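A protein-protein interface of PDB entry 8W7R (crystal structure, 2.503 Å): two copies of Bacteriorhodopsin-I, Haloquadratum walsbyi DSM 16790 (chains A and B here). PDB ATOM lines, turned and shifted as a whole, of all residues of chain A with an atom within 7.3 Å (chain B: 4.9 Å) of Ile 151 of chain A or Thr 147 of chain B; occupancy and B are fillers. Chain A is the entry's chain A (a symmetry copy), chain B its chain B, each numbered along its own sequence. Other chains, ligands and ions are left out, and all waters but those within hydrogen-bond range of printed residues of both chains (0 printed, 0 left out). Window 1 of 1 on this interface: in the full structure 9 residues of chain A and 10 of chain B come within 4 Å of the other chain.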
ATOM      1  N   ILE A 122     -21.350  -3.533 -16.531  1.00  0.00           N
ATOM      2  CA  ILE A 122     -20.033  -3.645 -15.912  1.00  0.00           C
ATOM      3  C   ILE A 122     -19.748  -2.412 -15.050  1.00  0.00           C
ATOM      4  O   ILE A 122     -19.235  -2.539 -13.935  1.00  0.00           O
ATOM      5  CB  ILE A 122     -18.932  -3.876 -16.956  1.00  0.00           C
ATOM      6  CG1 ILE A 122     -19.211  -5.124 -17.803  1.00  0.00           C
ATOM      7  CG2 ILE A 122     -17.575  -3.985 -16.259  1.00  0.00           C
ATOM      8  CD1 ILE A 122     -18.243  -5.313 -18.963  1.00  0.00           C
ATOM      9  N   PHE A 125     -21.603  -2.484 -11.774  1.00  0.00           N
ATOM     10  CA  PHE A 125     -20.884  -3.431 -10.937  1.00  0.00           C
ATOM     11  C   PHE A 125     -19.656  -2.764 -10.300  1.00  0.00           C
ATOM     12  O   PHE A 125     -19.424  -2.874  -9.094  1.00  0.00           O
ATOM     13  CB  PHE A 125     -20.496  -4.655 -11.777  1.00  0.00           C
ATOM     14  CG  PHE A 125     -19.828  -5.781 -10.998  1.00  0.00           C
ATOM     15  CD1 PHE A 125     -18.450  -5.790 -10.774  1.00  0.00           C
ATOM     16  CD2 PHE A 125     -20.581  -6.847 -10.514  1.00  0.00           C
ATOM     17  CE1 PHE A 125     -17.834  -6.847 -10.095  1.00  0.00           C
ATOM     18  CE2 PHE A 125     -19.968  -7.902  -9.831  1.00  0.00           C
ATOM     19  CZ  PHE A 125     -18.592  -7.901  -9.614  1.00  0.00           C
ATOM     20  N   MET A 126     -18.859  -2.087 -11.136  1.00  0.00           N
ATOM     21  CA  MET A 126     -17.694  -1.354 -10.674  1.00  0.00           C
ATOM     22  C   MET A 126     -18.043  -0.394  -9.531  1.00  0.00           C
ATOM     23  O   MET A 126     -17.426  -0.468  -8.459  1.00  0.00           O
ATOM     24  CB  MET A 126     -17.050  -0.601 -11.840  1.00  0.00           C
ATOM     25  CG  MET A 126     -15.763   0.099 -11.489  1.00  0.00           C
ATOM     26  SD  MET A 126     -15.166   1.036 -12.911  1.00  0.00           S
ATOM     27  CE  MET A 126     -16.549   2.135 -13.240  1.00  0.00           C
ATOM     28  N   ALA A 144     -10.862  -6.745  -0.686  1.00  0.00           N
ATOM     29  CA  ALA A 144     -11.333  -7.741  -1.629  1.00  0.00           C
ATOM     30  C   ALA A 144     -12.341  -7.101  -2.583  1.00  0.00           C
ATOM     31  O   ALA A 144     -12.316  -7.354  -3.787  1.00  0.00           O
ATOM     32  CB  ALA A 144     -11.914  -8.930  -0.891  1.00  0.00           C
ATOM     33  N   PHE A 145     -13.218  -6.249  -2.033  1.00  0.00           N
ATOM     34  CA  PHE A 145     -14.237  -5.604  -2.850  1.00  0.00           C
ATOM     35  C   PHE A 145     -13.559  -4.597  -3.771  1.00  0.00           C
ATOM     36  O   PHE A 145     -13.823  -4.550  -4.973  1.00  0.00           O
ATOM     37  CB  PHE A 145     -15.397  -5.009  -2.037  1.00  0.00           C
ATOM     38  CG  PHE A 145     -16.372  -6.052  -1.495  1.00  0.00           C
ATOM     39  CD1 PHE A 145     -17.118  -6.845  -2.368  1.00  0.00           C
ATOM     40  CD2 PHE A 145     -16.569  -6.203  -0.119  1.00  0.00           C
ATOM     41  CE1 PHE A 145     -18.008  -7.787  -1.873  1.00  0.00           C
ATOM     42  CE2 PHE A 145     -17.474  -7.139   0.375  1.00  0.00           C
ATOM     43  CZ  PHE A 145     -18.198  -7.921  -0.506  1.00  0.00           C
ATOM     44  N   TRP A 146     -12.651  -3.815  -3.191  1.00  0.00           N
ATOM     45  CA  TRP A 146     -11.889  -2.874  -3.989  1.00  0.00           C
ATOM     46  C   TRP A 146     -11.202  -3.578  -5.171  1.00  0.00           C
ATOM     47  O   TRP A 146     -11.216  -3.045  -6.279  1.00  0.00           O
ATOM     48  CB  TRP A 146     -10.909  -2.093  -3.101  1.00  0.00           C
ATOM     49  CG  TRP A 146      -9.973  -1.223  -3.896  1.00  0.00           C
ATOM     50  CD1 TRP A 146     -10.167   0.077  -4.265  1.00  0.00           C
ATOM     51  CD2 TRP A 146      -8.689  -1.612  -4.430  1.00  0.00           C
ATOM     52  NE1 TRP A 146      -9.097   0.529  -4.990  1.00  0.00           N
ATOM     53  CE2 TRP A 146      -8.172  -0.481  -5.107  1.00  0.00           C
ATOM     54  CE3 TRP A 146      -7.927  -2.786  -4.395  1.00  0.00           C
ATOM     55  CZ2 TRP A 146      -6.926  -0.494  -5.741  1.00  0.00           C
ATOM     56  CZ3 TRP A 146      -6.693  -2.788  -5.015  1.00  0.00           C
ATOM     57  CH2 TRP A 146      -6.199  -1.658  -5.674  1.00  0.00           C
ATOM     58  N   THR A 147     -10.651  -4.790  -4.941  1.00  0.00           N
ATOM     59  CA  THR A 147      -9.929  -5.566  -5.945  1.00  0.00           C
ATOM     60  C   THR A 147     -10.865  -6.010  -7.069  1.00  0.00           C
ATOM     61  O   THR A 147     -10.550  -5.844  -8.250  1.00  0.00           O
ATOM     62  CB  THR A 147      -9.246  -6.775  -5.298  1.00  0.00           C
ATOM     63  OG1 THR A 147      -8.332  -6.274  -4.325  1.00  0.00           O
ATOM     64  CG2 THR A 147      -8.514  -7.655  -6.299  1.00  0.00           C
ATOM     65  N   ILE A 148     -12.001  -6.608  -6.672  1.00  0.00           N
ATOM     66  CA  ILE A 148     -13.031  -7.075  -7.592  1.00  0.00           C
ATOM     67  C   ILE A 148     -13.488  -5.914  -8.478  1.00  0.00           C
ATOM     68  O   ILE A 148     -13.558  -6.049  -9.705  1.00  0.00           O
ATOM     69  CB  ILE A 148     -14.195  -7.747  -6.831  1.00  0.00           C
ATOM     70  CG1 ILE A 148     -13.712  -9.042  -6.155  1.00  0.00           C
ATOM     71  CG2 ILE A 148     -15.370  -8.029  -7.769  1.00  0.00           C
ATOM     72  CD1 ILE A 148     -14.607  -9.532  -5.025  1.00  0.00           C
ATOM     73  N   SER A 149     -13.759  -4.772  -7.834  1.00  0.00           N
ATOM     74  CA  SER A 149     -14.104  -3.550  -8.548  1.00  0.00           C
ATOM     75  C   SER A 149     -13.017  -3.174  -9.574  1.00  0.00           C
ATOM     76  O   SER A 149     -13.316  -2.952 -10.755  1.00  0.00           O
ATOM     77  CB  SER A 149     -14.405  -2.434  -7.564  1.00  0.00           C
ATOM     78  OG  SER A 149     -14.774  -1.215  -8.202  1.00  0.00           O
ATOM     79  N   THR A 150     -11.748  -3.168  -9.139  1.00  0.00           N
ATOM     80  CA  THR A 150     -10.666  -2.749 -10.018  1.00  0.00           C
ATOM     81  C   THR A 150     -10.555  -3.690 -11.219  1.00  0.00           C
ATOM     82  O   THR A 150     -10.334  -3.230 -12.346  1.00  0.00           O
ATOM     83  CB  THR A 150      -9.347  -2.604  -9.258  1.00  0.00           C
ATOM     84  OG1 THR A 150      -9.545  -1.768  -8.120  1.00  0.00           O
ATOM     85  CG2 THR A 150      -8.267  -1.995 -10.135  1.00  0.00           C
ATOM     86  N   ILE A 151     -10.717  -5.003 -10.959  1.00  0.00           N
ATOM     87  CA  ILE A 151     -10.720  -6.015 -12.008  1.00  0.00           C
ATOM     88  C   ILE A 151     -11.813  -5.690 -13.031  1.00  0.00           C
ATOM     89  O   ILE A 151     -11.550  -5.681 -14.236  1.00  0.00           O
ATOM     90  CB  ILE A 151     -10.913  -7.442 -11.469  1.00  0.00           C
ATOM     91  CG1 ILE A 151      -9.872  -7.839 -10.425  1.00  0.00           C
ATOM     92  CG2 ILE A 151     -10.989  -8.433 -12.628  1.00  0.00           C
ATOM     93  CD1 ILE A 151      -8.454  -7.475 -10.802  1.00  0.00           C
ATOM     94  N   SER A 152     -13.044  -5.435 -12.547  1.00  0.00           N
ATOM     95  CA  SER A 152     -14.163  -5.149 -13.437  1.00  0.00           C
ATOM     96  C   SER A 152     -13.927  -3.846 -14.226  1.00  0.00           C
ATOM     97  O   SER A 152     -14.319  -3.743 -15.398  1.00  0.00           O
ATOM     98  CB  SER A 152     -15.497  -5.183 -12.710  1.00  0.00           C
ATOM     99  OG  SER A 152     -15.795  -3.955 -12.043  1.00  0.00           O
ATOM    100  N   MET A 153     -13.242  -2.867 -13.607  1.00  0.00           N
ATOM    101  CA  MET A 153     -12.889  -1.652 -14.335  1.00  0.00           C
ATOM    102  C   MET A 153     -12.053  -2.008 -15.568  1.00  0.00           C
ATOM    103  O   MET A 153     -12.202  -1.378 -16.621  1.00  0.00           O
ATOM    104  CB  MET A 153     -12.126  -0.647 -13.459  1.00  0.00           C
ATOM    105  CG  MET A 153     -11.807   0.665 -14.158  1.00  0.00           C
ATOM    106  SD  MET A 153     -10.618   1.762 -13.357  1.00  0.00           S
ATOM    107  CE  MET A 153      -9.191   0.668 -13.324  1.00  0.00           C
ATOM    108  N   VAL A 154     -11.178  -3.024 -15.425  1.00  0.00           N
ATOM    109  CA  VAL A 154     -10.272  -3.424 -16.488  1.00  0.00           C
ATOM    110  C   VAL A 154     -11.062  -4.027 -17.646  1.00  0.00           C
ATOM    111  O   VAL A 154     -10.820  -3.682 -18.805  1.00  0.00           O
ATOM    112  CB  VAL A 154      -9.148  -4.350 -15.981  1.00  0.00           C
ATOM    113  CG1 VAL A 154      -8.442  -5.083 -17.119  1.00  0.00           C
ATOM    114  CG2 VAL A 154      -8.141  -3.580 -15.132  1.00  0.00           C
ATOM    115  N   PHE A 155     -11.998  -4.933 -17.331  1.00  0.00           N
ATOM    116  CA  PHE A 155     -12.895  -5.456 -18.354  1.00  0.00           C
ATOM    117  C   PHE A 155     -13.632  -4.298 -19.039  1.00  0.00           C
ATOM    118  O   PHE A 155     -13.759  -4.273 -20.266  1.00  0.00           O
ATOM    119  CB  PHE A 155     -13.869  -6.545 -17.885  1.00  0.00           C
ATOM    120  CG  PHE A 155     -13.202  -7.852 -17.492  1.00  0.00           C
ATOM    121  CD1 PHE A 155     -12.627  -8.007 -16.236  1.00  0.00           C
ATOM    122  CD2 PHE A 155     -13.140  -8.918 -18.385  1.00  0.00           C
ATOM    123  CE1 PHE A 155     -12.005  -9.198 -15.879  1.00  0.00           C
ATOM    124  CE2 PHE A 155     -12.521 -10.108 -18.028  1.00  0.00           C
ATOM    125  CZ  PHE A 155     -11.975 -10.252 -16.767  1.00  0.00           C
ATOM    126  N   LEU A 156     -14.108  -3.332 -18.239  1.00  0.00           N
ATOM    127  CA  LEU A 156     -14.826  -2.192 -18.794  1.00  0.00           C
ATOM    128  C   LEU A 156     -13.954  -1.489 -19.836  1.00  0.00           C
ATOM    129  O   LEU A 156     -14.372  -1.349 -20.989  1.00  0.00           O
ATOM    130  CB  LEU A 156     -15.275  -1.237 -17.690  1.00  0.00           C
ATOM    131  CG  LEU A 156     -16.030   0.021 -18.127  1.00  0.00           C
ATOM    132  CD1 LEU A 156     -17.278  -0.338 -18.915  1.00  0.00           C
ATOM    133  CD2 LEU A 156     -16.414   0.830 -16.897  1.00  0.00           C
ATOM    134  N   LEU A 157     -12.734  -1.104 -19.421  1.00  0.00           N
ATOM    135  CA  LEU A 157     -11.844  -0.285 -20.235  1.00  0.00           C
ATOM    136  C   LEU A 157     -11.438  -1.054 -21.491  1.00  0.00           C
ATOM    137  O   LEU A 157     -11.350  -0.479 -22.578  1.00  0.00           O
ATOM    138  CB  LEU A 157     -10.631   0.175 -19.430  1.00  0.00           C
ATOM    139  CG  LEU A 157     -10.971   1.074 -18.238  1.00  0.00           C
ATOM    140  CD1 LEU A 157      -9.792   1.322 -17.301  1.00  0.00           C
ATOM    141  CD2 LEU A 157     -11.574   2.378 -18.746  1.00  0.00           C
ATOM    142  N   TYR B 143      -4.573  -8.232 -19.371  1.00  0.00           N
ATOM    143  CA  TYR B 143      -4.643  -7.015 -18.572  1.00  0.00           C
ATOM    144  C   TYR B 143      -5.249  -7.303 -17.196  1.00  0.00           C
ATOM    145  O   TYR B 143      -4.878  -6.674 -16.200  1.00  0.00           O
ATOM    146  CB  TYR B 143      -5.343  -5.885 -19.336  1.00  0.00           C
ATOM    147  CG  TYR B 143      -4.528  -5.373 -20.517  1.00  0.00           C
ATOM    148  CD1 TYR B 143      -3.430  -4.543 -20.312  1.00  0.00           C
ATOM    149  CD2 TYR B 143      -4.861  -5.699 -21.835  1.00  0.00           C
ATOM    150  CE1 TYR B 143      -2.693  -4.055 -21.378  1.00  0.00           C
ATOM    151  CE2 TYR B 143      -4.123  -5.225 -22.906  1.00  0.00           C
ATOM    152  CZ  TYR B 143      -3.032  -4.406 -22.675  1.00  0.00           C
ATOM    153  OH  TYR B 143      -2.284  -3.933 -23.720  1.00  0.00           O
ATOM    154  N   ALA B 144      -6.170  -8.271 -17.143  1.00  0.00           N
ATOM    155  CA  ALA B 144      -6.770  -8.629 -15.870  1.00  0.00           C
ATOM    156  C   ALA B 144      -5.699  -9.246 -14.970  1.00  0.00           C
ATOM    157  O   ALA B 144      -5.646  -8.967 -13.777  1.00  0.00           O
ATOM    158  CB  ALA B 144      -7.949  -9.564 -16.079  1.00  0.00           C
ATOM    159  N   PHE B 145      -4.837 -10.087 -15.559  1.00  0.00           N
ATOM    160  CA  PHE B 145      -3.804 -10.748 -14.779  1.00  0.00           C
ATOM    161  C   PHE B 145      -2.760  -9.721 -14.373  1.00  0.00           C
ATOM    162  O   PHE B 145      -2.346  -9.676 -13.219  1.00  0.00           O
ATOM    163  CB  PHE B 145      -3.226 -11.980 -15.472  1.00  0.00           C
ATOM    164  CG  PHE B 145      -4.127 -13.204 -15.408  1.00  0.00           C
ATOM    165  CD1 PHE B 145      -4.416 -13.806 -14.181  1.00  0.00           C
ATOM    166  CD2 PHE B 145      -4.639 -13.775 -16.580  1.00  0.00           C
ATOM    167  CE1 PHE B 145      -5.251 -14.919 -14.121  1.00  0.00           C
ATOM    168  CE2 PHE B 145      -5.464 -14.890 -16.520  1.00  0.00           C
ATOM    169  CZ  PHE B 145      -5.768 -15.462 -15.287  1.00  0.00           C
ATOM    170  N   TRP B 146      -2.378  -8.870 -15.324  1.00  0.00           N
ATOM    171  CA  TRP B 146      -1.460  -7.791 -15.003  1.00  0.00           C
ATOM    172  C   TRP B 146      -1.971  -6.982 -13.809  1.00  0.00           C
ATOM    173  O   TRP B 146      -1.182  -6.663 -12.919  1.00  0.00           O
ATOM    174  CB  TRP B 146      -1.185  -6.914 -16.233  1.00  0.00           C
ATOM    175  CG  TRP B 146      -0.355  -5.696 -15.913  1.00  0.00           C
ATOM    176  CD1 TRP B 146       1.005  -5.608 -15.946  1.00  0.00           C
ATOM    177  CD2 TRP B 146      -0.832  -4.402 -15.469  1.00  0.00           C
ATOM    178  NE1 TRP B 146       1.412  -4.353 -15.586  1.00  0.00           N
ATOM    179  CE2 TRP B 146       0.311  -3.593 -15.272  1.00  0.00           C
ATOM    180  CE3 TRP B 146      -2.098  -3.852 -15.231  1.00  0.00           C
ATOM    181  CZ2 TRP B 146       0.218  -2.264 -14.849  1.00  0.00           C
ATOM    182  CZ3 TRP B 146      -2.187  -2.548 -14.783  1.00  0.00           C
ATOM    183  CH2 TRP B 146      -1.043  -1.759 -14.606  1.00  0.00           C
ATOM    184  N   THR B 147      -3.292  -6.705 -13.774  1.00  0.00           N
ATOM    185  CA  THR B 147      -3.926  -5.893 -12.739  1.00  0.00           C
ATOM    186  C   THR B 147      -3.861  -6.583 -11.380  1.00  0.00           C
ATOM    187  O   THR B 147      -3.456  -5.979 -10.391  1.00  0.00           O
ATOM    188  CB  THR B 147      -5.371  -5.568 -13.117  1.00  0.00           C
ATOM    189  OG1 THR B 147      -5.328  -4.874 -14.361  1.00  0.00           O
ATOM    190  CG2 THR B 147      -6.025  -4.695 -12.063  1.00  0.00           C
ATOM    191  N   ILE B 148      -4.290  -7.848 -11.352  1.00  0.00           N
ATOM    192  CA  ILE B 148      -4.264  -8.697 -10.165  1.00  0.00           C
ATOM    193  C   ILE B 148      -2.843  -8.749  -9.603  1.00  0.00           C
ATOM    194  O   ILE B 148      -2.632  -8.560  -8.404  1.00  0.00           O
ATOM    195  CB  ILE B 148      -4.810 -10.104 -10.493  1.00  0.00           C
ATOM    196  CG1 ILE B 148      -6.297 -10.059 -10.898  1.00  0.00           C
ATOM    197  CG2 ILE B 148      -4.594 -11.062  -9.325  1.00  0.00           C
ATOM    198  CD1 ILE B 148      -6.786 -11.308 -11.618  1.00  0.00           C
ATOM    199  N   SER B 149      -1.865  -8.961 -10.486  1.00  0.00           N
ATOM    200  CA  SER B 149      -0.462  -8.961 -10.104  1.00  0.00           C
ATOM    201  C   SER B 149      -0.066  -7.628  -9.458  1.00  0.00           C
ATOM    202  O   SER B 149       0.496  -7.593  -8.358  1.00  0.00           O
ATOM    203  CB  SER B 149       0.401  -9.314 -11.306  1.00  0.00           C
ATOM    204  OG  SER B 149       1.772  -9.410 -10.956  1.00  0.00           O
ATOM    205  N   THR B 150      -0.433  -6.520 -10.115  1.00  0.00           N
ATOM    206  CA  THR B 150      -0.047  -5.196  -9.644  1.00  0.00           C
ATOM    207  C   THR B 150      -0.681  -4.918  -8.287  1.00  0.00           C
ATOM    208  O   THR B 150      -0.015  -4.343  -7.423  1.00  0.00           O
ATOM    209  CB  THR B 150      -0.371  -4.106 -10.665  1.00  0.00           C
ATOM    210  OG1 THR B 150       0.265  -4.500 -11.875  1.00  0.00           O
ATOM    211  CG2 THR B 150       0.208  -2.768 -10.250  1.00  0.00           C
ATOM    212  N   ILE B 151      -1.955  -5.338  -8.126  1.00  0.00           N
ATOM    213  CA  ILE B 151      -2.667  -5.247  -6.858  1.00  0.00           C
ATOM    214  C   ILE B 151      -1.856  -5.960  -5.785  1.00  0.00           C
ATOM    215  O   ILE B 151      -1.627  -5.375  -4.728  1.00  0.00           O
ATOM    216  CB  ILE B 151      -4.101  -5.824  -6.921  1.00  0.00           C
ATOM    217  CG1 ILE B 151      -4.986  -5.092  -7.914  1.00  0.00           C
ATOM    218  CG2 ILE B 151      -4.742  -5.891  -5.534  1.00  0.00           C
ATOM    219  CD1 ILE B 151      -4.796  -3.594  -7.907  1.00  0.00           C
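OG1 of Thr 147 of chain B is in hydrogen-bond range of O of Tyr 143 of chain B (2.6 Å). O of Trp 146 of chain A is in hydrogen-bond range of OG1 of Thr 150 of chain A (2.8 Å).
Trp 146 of chain A touches Ile 151 of chain B, but with the chains exchanged Ile 151 of chain A does not touch Trp 146 of chain B (7.2 Å). Thr 147 of chain A touches Ile 151 of chain B, and with the chains exchanged Ile 151 of chain A touches Thr 147 of chain B. Ile 151 of chain A touches Ile 148 of chain B, but with the chains exchanged Ile 148 of chain A does not touch Ile 151 of chain B (7.3 Å).
Of the 9 printed residues of chain B, 5 touch a printed residue of chain A. Hydrophobic or aromatic side chains of chain B that line the printed part of chain A: Tyr 143, Ile 148 and Ile 151.
Among the printed residues, merely in contact across the chains: Trp 146 of chain A with Ile 151 of chain B (3.3 Å), Thr 147 of chain A with Ile 151 of chain B (3.8 Å), Ile 151 of chain A with Thr 147 of chain B (3.9 Å), Ile 151 of chain A with Ile 148 of chain B (3.4 Å), Val 154 of chain A with Tyr 143 of chain B (3.9 Å), Val 154 of chain A with Ala 144 of chain B (3.9 Å) and Val 154 of chain A with Thr 147 of chain B (3.2 Å).
Of the printed residues of chain B, Trp 146 of chain A touches Ile 151. Ile 151 of chain A touches just these residues of chain B: Thr 147 (3.9 Å) and Ile 148 (3.4 Å). Of the printed residues of chain B, Val 154 of chain A touches Tyr 143 (3.9 Å), Ala 144 (3.9 Å) and Thr 147 (3.2 Å). Of the printed residues of chain A, Tyr 143 of chain B touches Val 154 (3.9 Å). Of the printed residues of chain A, Ala 144 of chain B touches Val 154. Printed residues of chain A within 4 Å of Thr 147 of chain B: Ile 151 (3.9 Å) and Val 154 (3.2 Å). The nearest printed residue of chain A that does not touch Thr 147 of chain B is Thr 150 of chain A (4.004 Å). The nearest printed residue of chain B that does not touch Val 154 of chain A is Trp 146 of chain B (6.0 Å).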
